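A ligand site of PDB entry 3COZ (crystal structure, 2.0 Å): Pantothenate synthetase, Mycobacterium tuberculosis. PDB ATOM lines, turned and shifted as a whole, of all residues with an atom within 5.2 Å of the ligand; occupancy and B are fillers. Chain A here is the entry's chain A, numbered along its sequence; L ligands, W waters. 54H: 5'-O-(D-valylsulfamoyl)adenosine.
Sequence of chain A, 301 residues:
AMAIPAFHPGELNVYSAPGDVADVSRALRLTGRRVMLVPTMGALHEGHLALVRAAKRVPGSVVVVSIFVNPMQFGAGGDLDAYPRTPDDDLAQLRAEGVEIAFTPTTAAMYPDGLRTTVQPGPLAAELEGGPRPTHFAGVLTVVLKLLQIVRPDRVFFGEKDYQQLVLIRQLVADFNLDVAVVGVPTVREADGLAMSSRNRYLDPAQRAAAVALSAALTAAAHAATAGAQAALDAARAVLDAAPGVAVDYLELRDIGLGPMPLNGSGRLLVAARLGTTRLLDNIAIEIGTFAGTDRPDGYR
OD2 of Asp 162 is in hydrogen-bond range of O2' of the ligand (2.7 Å).
N of Gly 159 lies within hydrogen-bond range of O3' of the ligand.
The backbone carbonyl oxygen (O) of Val 188 is in hydrogen-bond range of a nitrogen (N6) of the ligand.
The side-chain amide oxygen of Gln 73 sits at hydrogen-bond distance from a nitrogen (N) of the ligand (3.1 Å).
N1 of the ligand sits at hydrogen-bond distance from N of Val 188 (2.9 Å).
OAG of the ligand is in hydrogen-bond range of NE2 of His 48 (3.1 Å).
A nitrogen (N) of the ligand lies within hydrogen-bond range of the side-chain amide oxygen (OE1) of Gln 165.
An oxygen (OAG) of the ligand sits at hydrogen-bond distance from the backbone NH of Met 41 (2.9 Å).
The backbone carbonyl oxygen (O) of Met 196 is in hydrogen-bond range of a nitrogen (N6) of the ligand (2.8 Å).
The backbone carbonyl oxygen of Val 188 lies within hydrogen-bond range of the backbone NH of Met 196, at 2.9 Å.
The backbone carbonyl oxygen (O) of Phe 158 is in hydrogen-bond range of the backbone NH (N) of Val 185 (2.9 Å).
OG1 of Thr 187 is in hydrogen-bond range of N of Lys 161 (3.0 Å).
The backbone NH (N) of His 45 is in hydrogen-bond range of a ring nitrogen (ND1) of His 48 (3.0 Å).
The backbone NH of Gly 47 sits at hydrogen-bond distance from a ring nitrogen (ND1) of His 45 (3.1 Å).
The side-chain amide oxygen of Gln 73 lies close to the side-chain sulfur of Met 41.
The backbone NH (N) of Gly 42 lies within hydrogen-bond range of the side-chain hydroxyl (OG1) of Thr 40, 3.1 Å away.
Water W2 lies within hydrogen-bond range of O of Pro 39 (2.6 Å), O of Phe 157 (2.7 Å) and O3' of the ligand (2.7 Å).
Water W1 lies within hydrogen-bond range of the backbone carbonyl oxygen of Asp 162 (2.7 Å), the backbone carbonyl oxygen of Gly 159 (2.8 Å), the side-chain amide nitrogen of Gln 165 (3.0 Å) and an oxygen (O2') of the ligand (3.3 Å).
Merely in contact with the ligand: Pro 39 (3.4 Å), Thr 40 (3.7 Å), His 45 (3.2 Å), Gly 47 (3.5 Å), Leu 51 (3.6 Å), Tyr 83 (3.6 Å), Phe 158 (3.2 Å), Lys 161 (3.8 Å), Pro 186 (3.7 Å) and Thr 187 (3.5 Å).
Of the 26 residues printed, 18 come within 4 Å of the ligand.
The nearest printed residue that does not touch the ligand is Val 140 (4.1 Å).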
ATOM      1  N   PRO A  39      13.360  -2.034 -12.032  1.00  0.00           N
ATOM      2  CA  PRO A  39      13.503  -0.845 -12.886  1.00  0.00           C
ATOM      3  C   PRO A  39      12.295  -0.676 -13.742  1.00  0.00           C
ATOM      4  O   PRO A  39      11.931  -1.607 -14.433  1.00  0.00           O
ATOM      5  CB  PRO A  39      14.703  -1.176 -13.759  1.00  0.00           C
ATOM      6  CG  PRO A  39      15.417  -2.355 -13.031  1.00  0.00           C
ATOM      7  CD  PRO A  39      14.226  -3.128 -12.495  1.00  0.00           C
ATOM      8  N   THR A  40      11.687   0.512 -13.696  1.00  0.00           N
ATOM      9  CA  THR A  40      10.538   0.860 -14.561  1.00  0.00           C
ATOM     10  C   THR A  40      10.686   2.253 -15.176  1.00  0.00           C
ATOM     11  O   THR A  40      11.522   3.067 -14.739  1.00  0.00           O
ATOM     12  CB  THR A  40       9.204   0.902 -13.759  1.00  0.00           C
ATOM     13  OG1 THR A  40       9.100   2.141 -13.064  1.00  0.00           O
ATOM     14  CG2 THR A  40       9.113  -0.244 -12.743  1.00  0.00           C
ATOM     15  N   MET A  41       9.866   2.525 -16.191  1.00  0.00           N
ATOM     16  CA  MET A  41       9.775   3.862 -16.781  1.00  0.00           C
ATOM     17  C   MET A  41       8.503   4.538 -16.327  1.00  0.00           C
ATOM     18  O   MET A  41       8.037   5.496 -16.942  1.00  0.00           O
ATOM     19  CB  MET A  41       9.851   3.797 -18.323  1.00  0.00           C
ATOM     20  CG  MET A  41      11.228   3.369 -18.806  1.00  0.00           C
ATOM     21  SD  MET A  41      11.647   3.880 -20.500  1.00  0.00           S
ATOM     22  CE  MET A  41      10.547   2.819 -21.414  1.00  0.00           C
ATOM     23  N   GLY A  42       7.911   4.032 -15.261  1.00  0.00           N
ATOM     24  CA  GLY A  42       6.655   4.595 -14.760  1.00  0.00           C
ATOM     25  C   GLY A  42       5.435   4.187 -15.570  1.00  0.00           C
ATOM     26  O   GLY A  42       5.507   3.253 -16.382  1.00  0.00           O
ATOM     27  N   HIS A  45       1.287  -0.405 -14.418  1.00  0.00           N
ATOM     28  CA  HIS A  45       0.087  -1.213 -14.551  1.00  0.00           C
ATOM     29  C   HIS A  45       0.314  -2.587 -13.899  1.00  0.00           C
ATOM     30  O   HIS A  45       1.355  -2.832 -13.272  1.00  0.00           O
ATOM     31  CB  HIS A  45      -0.355  -1.316 -16.029  1.00  0.00           C
ATOM     32  CG  HIS A  45       0.713  -1.831 -16.949  1.00  0.00           C
ATOM     33  ND1 HIS A  45       1.234  -3.105 -16.841  1.00  0.00           N
ATOM     34  CD2 HIS A  45       1.305  -1.278 -18.040  1.00  0.00           C
ATOM     35  CE1 HIS A  45       2.145  -3.293 -17.789  1.00  0.00           C
ATOM     36  NE2 HIS A  45       2.186  -2.203 -18.547  1.00  0.00           N
ATOM     37  N   GLY A  47       1.126  -5.483 -14.931  1.00  0.00           N
ATOM     38  CA  GLY A  47       2.339  -6.152 -15.361  1.00  0.00           C
ATOM     39  C   GLY A  47       3.544  -5.711 -14.531  1.00  0.00           C
ATOM     40  O   GLY A  47       4.338  -6.527 -14.073  1.00  0.00           O
ATOM     41  N   HIS A  48       3.673  -4.394 -14.321  1.00  0.00           N
ATOM     42  CA  HIS A  48       4.752  -3.897 -13.467  1.00  0.00           C
ATOM     43  C   HIS A  48       4.565  -4.381 -12.028  1.00  0.00           C
ATOM     44  O   HIS A  48       5.551  -4.671 -11.345  1.00  0.00           O
ATOM     45  CB  HIS A  48       4.813  -2.370 -13.450  1.00  0.00           C
ATOM     46  CG  HIS A  48       5.005  -1.754 -14.797  1.00  0.00           C
ATOM     47  ND1 HIS A  48       3.985  -1.114 -15.461  1.00  0.00           N
ATOM     48  CD2 HIS A  48       6.089  -1.685 -15.610  1.00  0.00           C
ATOM     49  CE1 HIS A  48       4.430  -0.649 -16.620  1.00  0.00           C
ATOM     50  NE2 HIS A  48       5.711  -0.973 -16.724  1.00  0.00           N
ATOM     51  N   LEU A  51       6.037  -7.789 -11.002  1.00  0.00           N
ATOM     52  CA  LEU A  51       7.465  -7.708 -10.711  1.00  0.00           C
ATOM     53  C   LEU A  51       7.616  -7.226  -9.282  1.00  0.00           C
ATOM     54  O   LEU A  51       8.436  -7.755  -8.531  1.00  0.00           O
ATOM     55  CB  LEU A  51       8.200  -6.724 -11.625  1.00  0.00           C
ATOM     56  CG  LEU A  51       8.062  -6.659 -13.159  1.00  0.00           C
ATOM     57  CD1 LEU A  51       9.393  -6.236 -13.776  1.00  0.00           C
ATOM     58  CD2 LEU A  51       7.601  -7.927 -13.794  1.00  0.00           C
ATOM     59  N   GLN A  73      17.566   5.560 -24.574  1.00  0.00           N
ATOM     60  CA  GLN A  73      17.039   4.355 -25.226  1.00  0.00           C
ATOM     61  C   GLN A  73      15.970   4.660 -26.288  1.00  0.00           C
ATOM     62  O   GLN A  73      15.548   3.767 -27.034  1.00  0.00           O
ATOM     63  CB  GLN A  73      16.539   3.338 -24.203  1.00  0.00           C
ATOM     64  CG  GLN A  73      15.352   3.792 -23.337  1.00  0.00           C
ATOM     65  CD  GLN A  73      14.932   2.726 -22.319  1.00  0.00           C
ATOM     66  OE1 GLN A  73      13.960   1.993 -22.533  1.00  0.00           O
ATOM     67  NE2 GLN A  73      15.682   2.629 -21.212  1.00  0.00           N
ATOM     68  N   TYR A  83       6.048   9.337 -24.501  1.00  0.00           N
ATOM     69  CA  TYR A  83       5.953   8.303 -23.457  1.00  0.00           C
ATOM     70  C   TYR A  83       5.040   8.751 -22.311  1.00  0.00           C
ATOM     71  O   TYR A  83       5.203   9.864 -21.789  1.00  0.00           O
ATOM     72  CB  TYR A  83       7.336   7.873 -22.942  1.00  0.00           C
ATOM     73  CG  TYR A  83       7.258   6.534 -22.258  1.00  0.00           C
ATOM     74  CD1 TYR A  83       7.283   5.343 -23.008  1.00  0.00           C
ATOM     75  CD2 TYR A  83       7.092   6.429 -20.876  1.00  0.00           C
ATOM     76  CE1 TYR A  83       7.179   4.099 -22.400  1.00  0.00           C
ATOM     77  CE2 TYR A  83       6.978   5.181 -20.255  1.00  0.00           C
ATOM     78  CZ  TYR A  83       7.027   4.025 -21.021  1.00  0.00           C
ATOM     79  OH  TYR A  83       6.923   2.797 -20.416  1.00  0.00           O
ATOM     80  N   VAL A 140      19.321   1.165 -23.042  1.00  0.00           N
ATOM     81  CA  VAL A 140      18.748   0.341 -21.975  1.00  0.00           C
ATOM     82  C   VAL A 140      19.835  -0.229 -21.084  1.00  0.00           C
ATOM     83  O   VAL A 140      19.783  -0.075 -19.857  1.00  0.00           O
ATOM     84  CB  VAL A 140      17.922  -0.820 -22.583  1.00  0.00           C
ATOM     85  CG1 VAL A 140      17.477  -1.765 -21.512  1.00  0.00           C
ATOM     86  CG2 VAL A 140      16.727  -0.264 -23.396  1.00  0.00           C
ATOM     87  N   VAL A 144      20.433   0.571 -17.149  1.00  0.00           N
ATOM     88  CA  VAL A 144      20.307  -0.501 -16.191  1.00  0.00           C
ATOM     89  C   VAL A 144      21.635  -0.748 -15.436  1.00  0.00           C
ATOM     90  O   VAL A 144      21.626  -0.972 -14.221  1.00  0.00           O
ATOM     91  CB  VAL A 144      19.776  -1.810 -16.831  1.00  0.00           C
ATOM     92  CG1 VAL A 144      19.889  -2.982 -15.830  1.00  0.00           C
ATOM     93  CG2 VAL A 144      18.333  -1.637 -17.256  1.00  0.00           C
ATOM     94  N   PHE A 157      14.577  -7.418 -11.190  1.00  0.00           N
ATOM     95  CA  PHE A 157      13.384  -8.035 -11.792  1.00  0.00           C
ATOM     96  C   PHE A 157      13.017  -7.437 -13.168  1.00  0.00           C
ATOM     97  O   PHE A 157      12.922  -6.201 -13.306  1.00  0.00           O
ATOM     98  CB  PHE A 157      12.216  -7.931 -10.802  1.00  0.00           C
ATOM     99  CG  PHE A 157      12.441  -8.744  -9.565  1.00  0.00           C
ATOM    100  CD1 PHE A 157      13.289  -8.273  -8.537  1.00  0.00           C
ATOM    101  CD2 PHE A 157      11.889 -10.003  -9.449  1.00  0.00           C
ATOM    102  CE1 PHE A 157      13.554  -9.053  -7.380  1.00  0.00           C
ATOM    103  CE2 PHE A 157      12.136 -10.793  -8.278  1.00  0.00           C
ATOM    104  CZ  PHE A 157      12.978 -10.314  -7.268  1.00  0.00           C
ATOM    105  N   PHE A 158      12.809  -8.297 -14.159  1.00  0.00           N
ATOM    106  CA  PHE A 158      12.393  -7.860 -15.497  1.00  0.00           C
ATOM    107  C   PHE A 158      11.258  -8.750 -16.012  1.00  0.00           C
ATOM    108  O   PHE A 158      11.212  -9.932 -15.684  1.00  0.00           O
ATOM    109  CB  PHE A 158      13.588  -7.919 -16.476  1.00  0.00           C
ATOM    110  CG  PHE A 158      14.562  -6.783 -16.290  1.00  0.00           C
ATOM    111  CD1 PHE A 158      14.359  -5.561 -16.914  1.00  0.00           C
ATOM    112  CD2 PHE A 158      15.674  -6.930 -15.471  1.00  0.00           C
ATOM    113  CE1 PHE A 158      15.268  -4.487 -16.721  1.00  0.00           C
ATOM    114  CE2 PHE A 158      16.576  -5.878 -15.296  1.00  0.00           C
ATOM    115  CZ  PHE A 158      16.349  -4.659 -15.925  1.00  0.00           C
ATOM    116  N   GLY A 159      10.345  -8.203 -16.813  1.00  0.00           N
ATOM    117  CA  GLY A 159       9.221  -9.012 -17.342  1.00  0.00           C
ATOM    118  C   GLY A 159       9.595  -9.797 -18.575  1.00  0.00           C
ATOM    119  O   GLY A 159      10.457  -9.355 -19.350  1.00  0.00           O
ATOM    120  N   GLU A 160       8.957 -10.959 -18.788  1.00  0.00           N
ATOM    121  CA  GLU A 160       9.219 -11.719 -20.039  1.00  0.00           C
ATOM    122  C   GLU A 160       8.577 -11.032 -21.243  1.00  0.00           C
ATOM    123  O   GLU A 160       8.883 -11.365 -22.387  1.00  0.00           O
ATOM    124  CB  GLU A 160       8.715 -13.143 -19.911  1.00  0.00           C
ATOM    125  CG  GLU A 160       9.504 -13.998 -18.904  1.00  0.00           C
ATOM    126  CD  GLU A 160       8.997 -15.433 -18.825  1.00  0.00           C
ATOM    127  OE1 GLU A 160       7.955 -15.762 -19.456  1.00  0.00           O
ATOM    128  OE2 GLU A 160       9.641 -16.218 -18.116  1.00  0.00           O
ATOM    129  N   LYS A 161       7.689 -10.077 -20.984  1.00  0.00           N
ATOM    130  CA  LYS A 161       7.016  -9.342 -22.063  1.00  0.00           C
ATOM    131  C   LYS A 161       8.077  -8.699 -22.958  1.00  0.00           C
ATOM    132  O   LYS A 161       8.043  -8.828 -24.178  1.00  0.00           O
ATOM    133  CB  LYS A 161       6.021  -8.297 -21.542  1.00  0.00           C
ATOM    134  CG  LYS A 161       5.407  -7.504 -22.731  1.00  0.00           C
ATOM    135  CD  LYS A 161       4.112  -6.843 -22.425  1.00  0.00           C
ATOM    136  CE  LYS A 161       3.744  -5.878 -23.544  1.00  0.00           C
ATOM    137  NZ  LYS A 161       4.460  -6.167 -24.825  1.00  0.00           N
ATOM    138  N   ASP A 162       9.058  -8.064 -22.341  1.00  0.00           N
ATOM    139  CA  ASP A 162      10.205  -7.589 -23.076  1.00  0.00           C
ATOM    140  C   ASP A 162      11.323  -8.624 -23.026  1.00  0.00           C
ATOM    141  O   ASP A 162      12.330  -8.426 -22.361  1.00  0.00           O
ATOM    142  CB  ASP A 162      10.583  -6.220 -22.528  1.00  0.00           C
ATOM    143  CG  ASP A 162       9.444  -5.236 -22.674  1.00  0.00           C
ATOM    144  OD1 ASP A 162       9.248  -4.770 -23.800  1.00  0.00           O
ATOM    145  OD2 ASP A 162       8.687  -5.014 -21.695  1.00  0.00           O
ATOM    146  N   GLN A 165      14.935  -7.759 -24.230  1.00  0.00           N
ATOM    147  CA  GLN A 165      15.543  -6.941 -23.192  1.00  0.00           C
ATOM    148  C   GLN A 165      16.059  -7.803 -22.022  1.00  0.00           C
ATOM    149  O   GLN A 165      17.168  -7.611 -21.557  1.00  0.00           O
ATOM    150  CB  GLN A 165      14.486  -5.979 -22.651  1.00  0.00           C
ATOM    151  CG  GLN A 165      14.951  -5.180 -21.468  1.00  0.00           C
ATOM    152  CD  GLN A 165      13.985  -4.070 -21.181  1.00  0.00           C
ATOM    153  OE1 GLN A 165      14.131  -2.970 -21.730  1.00  0.00           O
ATOM    154  NE2 GLN A 165      12.968  -4.359 -20.363  1.00  0.00           N
ATOM    155  N   VAL A 185      10.009 -12.439 -14.872  1.00  0.00           N
ATOM    156  CA  VAL A 185       8.674 -12.638 -14.315  1.00  0.00           C
ATOM    157  C   VAL A 185       7.710 -12.827 -15.487  1.00  0.00           C
ATOM    158  O   VAL A 185       7.788 -12.086 -16.484  1.00  0.00           O
ATOM    159  CB  VAL A 185       8.286 -11.423 -13.449  1.00  0.00           C
ATOM    160  CG1 VAL A 185       6.889 -11.597 -12.814  1.00  0.00           C
ATOM    161  CG2 VAL A 185       9.292 -11.203 -12.371  1.00  0.00           C
ATOM    162  N   PRO A 186       6.809 -13.856 -15.409  1.00  0.00           N
ATOM    163  CA  PRO A 186       5.921 -14.153 -16.552  1.00  0.00           C
ATOM    164  C   PRO A 186       5.045 -12.962 -16.917  1.00  0.00           C
ATOM    165  O   PRO A 186       4.691 -12.145 -16.046  1.00  0.00           O
ATOM    166  CB  PRO A 186       5.077 -15.323 -16.040  1.00  0.00           C
ATOM    167  CG  PRO A 186       5.958 -15.978 -15.010  1.00  0.00           C
ATOM    168  CD  PRO A 186       6.585 -14.815 -14.309  1.00  0.00           C
ATOM    169  N   THR A 187       4.748 -12.838 -18.207  1.00  0.00           N
ATOM    170  CA  THR A 187       3.911 -11.736 -18.730  1.00  0.00           C
ATOM    171  C   THR A 187       2.488 -11.707 -18.155  1.00  0.00           C
ATOM    172  O   THR A 187       1.804 -12.744 -18.101  1.00  0.00           O
ATOM    173  CB  THR A 187       3.804 -11.863 -20.258  1.00  0.00           C
ATOM    174  OG1 THR A 187       5.117 -11.701 -20.812  1.00  0.00           O
ATOM    175  CG2 THR A 187       2.844 -10.784 -20.851  1.00  0.00           C
ATOM    176  N   VAL A 188       2.029 -10.536 -17.733  1.00  0.00           N
ATOM    177  CA  VAL A 188       0.679 -10.406 -17.208  1.00  0.00           C
ATOM    178  C   VAL A 188      -0.237 -10.016 -18.367  1.00  0.00           C
ATOM    179  O   VAL A 188       0.098  -9.103 -19.159  1.00  0.00           O
ATOM    180  CB  VAL A 188       0.605  -9.386 -16.045  1.00  0.00           C
ATOM    181  CG1 VAL A 188      -0.842  -9.280 -15.497  1.00  0.00           C
ATOM    182  CG2 VAL A 188       1.559  -9.803 -14.947  1.00  0.00           C
ATOM    183  N   ALA A 195      -1.340  -9.069 -23.932  1.00  0.00           N
ATOM    184  CA  ALA A 195      -0.238  -8.709 -23.033  1.00  0.00           C
ATOM    185  C   ALA A 195      -0.434  -7.293 -22.536  1.00  0.00           C
ATOM    186  O   ALA A 195      -0.577  -6.372 -23.340  1.00  0.00           O
ATOM    187  CB  ALA A 195       1.075  -8.806 -23.725  1.00  0.00           C
ATOM    188  N   MET A 196      -0.412  -7.106 -21.228  1.00  0.00           N
ATOM    189  CA  MET A 196      -0.594  -5.770 -20.669  1.00  0.00           C
ATOM    190  C   MET A 196       0.568  -4.858 -21.040  1.00  0.00           C
ATOM    191  O   MET A 196       1.745  -5.250 -20.931  1.00  0.00           O
ATOM    192  CB  MET A 196      -0.745  -5.818 -19.163  1.00  0.00           C
ATOM    193  CG  MET A 196      -2.015  -6.465 -18.703  1.00  0.00           C
ATOM    194  SD  MET A 196      -2.392  -5.905 -17.052  1.00  0.00           S
ATOM    195  CE  MET A 196      -2.825  -4.215 -17.454  1.00  0.00           C
ATOM    196  N   SER A 197       0.254  -3.649 -21.493  1.00  0.00           N
ATOM    197  CA  SER A 197       1.282  -2.687 -21.841  1.00  0.00           C
ATOM    198  C   SER A 197       0.666  -1.305 -21.718  1.00  0.00           C
ATOM    199  O   SER A 197      -0.547  -1.147 -21.920  1.00  0.00           O
ATOM    200  CB  SER A 197       1.772  -2.889 -23.292  1.00  0.00           C
ATOM    201  OG  SER A 197       2.518  -1.760 -23.741  1.00  0.00           O
HETATM  202  C4  54H L   1       5.811  -6.440 -17.734  1.00  0.00           C
HETATM  203  C5  54H L   1       4.589  -6.229 -18.381  1.00  0.00           C
HETATM  204  C6  54H L   1       3.655  -7.264 -18.352  1.00  0.00           C
HETATM  205  C8  54H L   1       5.831  -4.466 -18.642  1.00  0.00           C
HETATM  206  N1  54H L   1       3.972  -8.404 -17.685  1.00  0.00           N
HETATM  207  N3  54H L   1       6.067  -7.601 -17.089  1.00  0.00           N
HETATM  208  CG2 54H L   1      13.690  -1.976 -17.847  1.00  0.00           C
HETATM  209  CB  54H L   1      13.906  -0.542 -18.317  1.00  0.00           C
HETATM  210  CG1 54H L   1      13.761   0.423 -17.143  1.00  0.00           C
HETATM  211  CA  54H L   1      12.954  -0.171 -19.472  1.00  0.00           C
HETATM  212  N   54H L   1      13.556  -0.494 -20.797  1.00  0.00           N
HETATM  213  C   54H L   1      11.514  -0.778 -19.360  1.00  0.00           C
HETATM  214  O   54H L   1      11.234  -1.829 -19.916  1.00  0.00           O
HETATM  215  NAP 54H L   1      10.633  -0.029 -18.678  1.00  0.00           N
HETATM  216  SBD 54H L   1       9.055  -0.441 -18.499  1.00  0.00           S
HETATM  217  OAF 54H L   1       8.438  -0.464 -19.857  1.00  0.00           O
HETATM  218  OAG 54H L   1       8.365   0.508 -17.542  1.00  0.00           O
HETATM  219  O5' 54H L   1       8.880  -1.785 -17.980  1.00  0.00           O
HETATM  220  C5' 54H L   1       9.445  -2.134 -16.690  1.00  0.00           C
HETATM  221  C4' 54H L   1       9.397  -3.636 -16.482  1.00  0.00           C
HETATM  222  O4' 54H L   1       7.999  -4.088 -16.488  1.00  0.00           O
HETATM  223  C3' 54H L   1      10.089  -4.303 -17.671  1.00  0.00           C
HETATM  224  O3' 54H L   1      10.853  -5.349 -17.143  1.00  0.00           O
HETATM  225  C2' 54H L   1       8.918  -4.862 -18.485  1.00  0.00           C
HETATM  226  O2' 54H L   1       9.265  -6.031 -19.258  1.00  0.00           O
HETATM  227  C1' 54H L   1       7.929  -5.192 -17.361  1.00  0.00           C
HETATM  228  N9  54H L   1       6.543  -5.348 -17.907  1.00  0.00           N
HETATM  229  N7  54H L   1       4.631  -5.006 -18.930  1.00  0.00           N
HETATM  230  C2  54H L   1       5.140  -8.565 -17.066  1.00  0.00           C
HETATM  231  N6  54H L   1       2.482  -7.142 -18.965  1.00  0.00           N
HETATM  232  O   HOH W   1      12.296  -7.286 -19.881  1.00  0.00           O
HETATM  233  O   HOH W   2      12.031  -4.198 -14.949  1.00  0.00           O
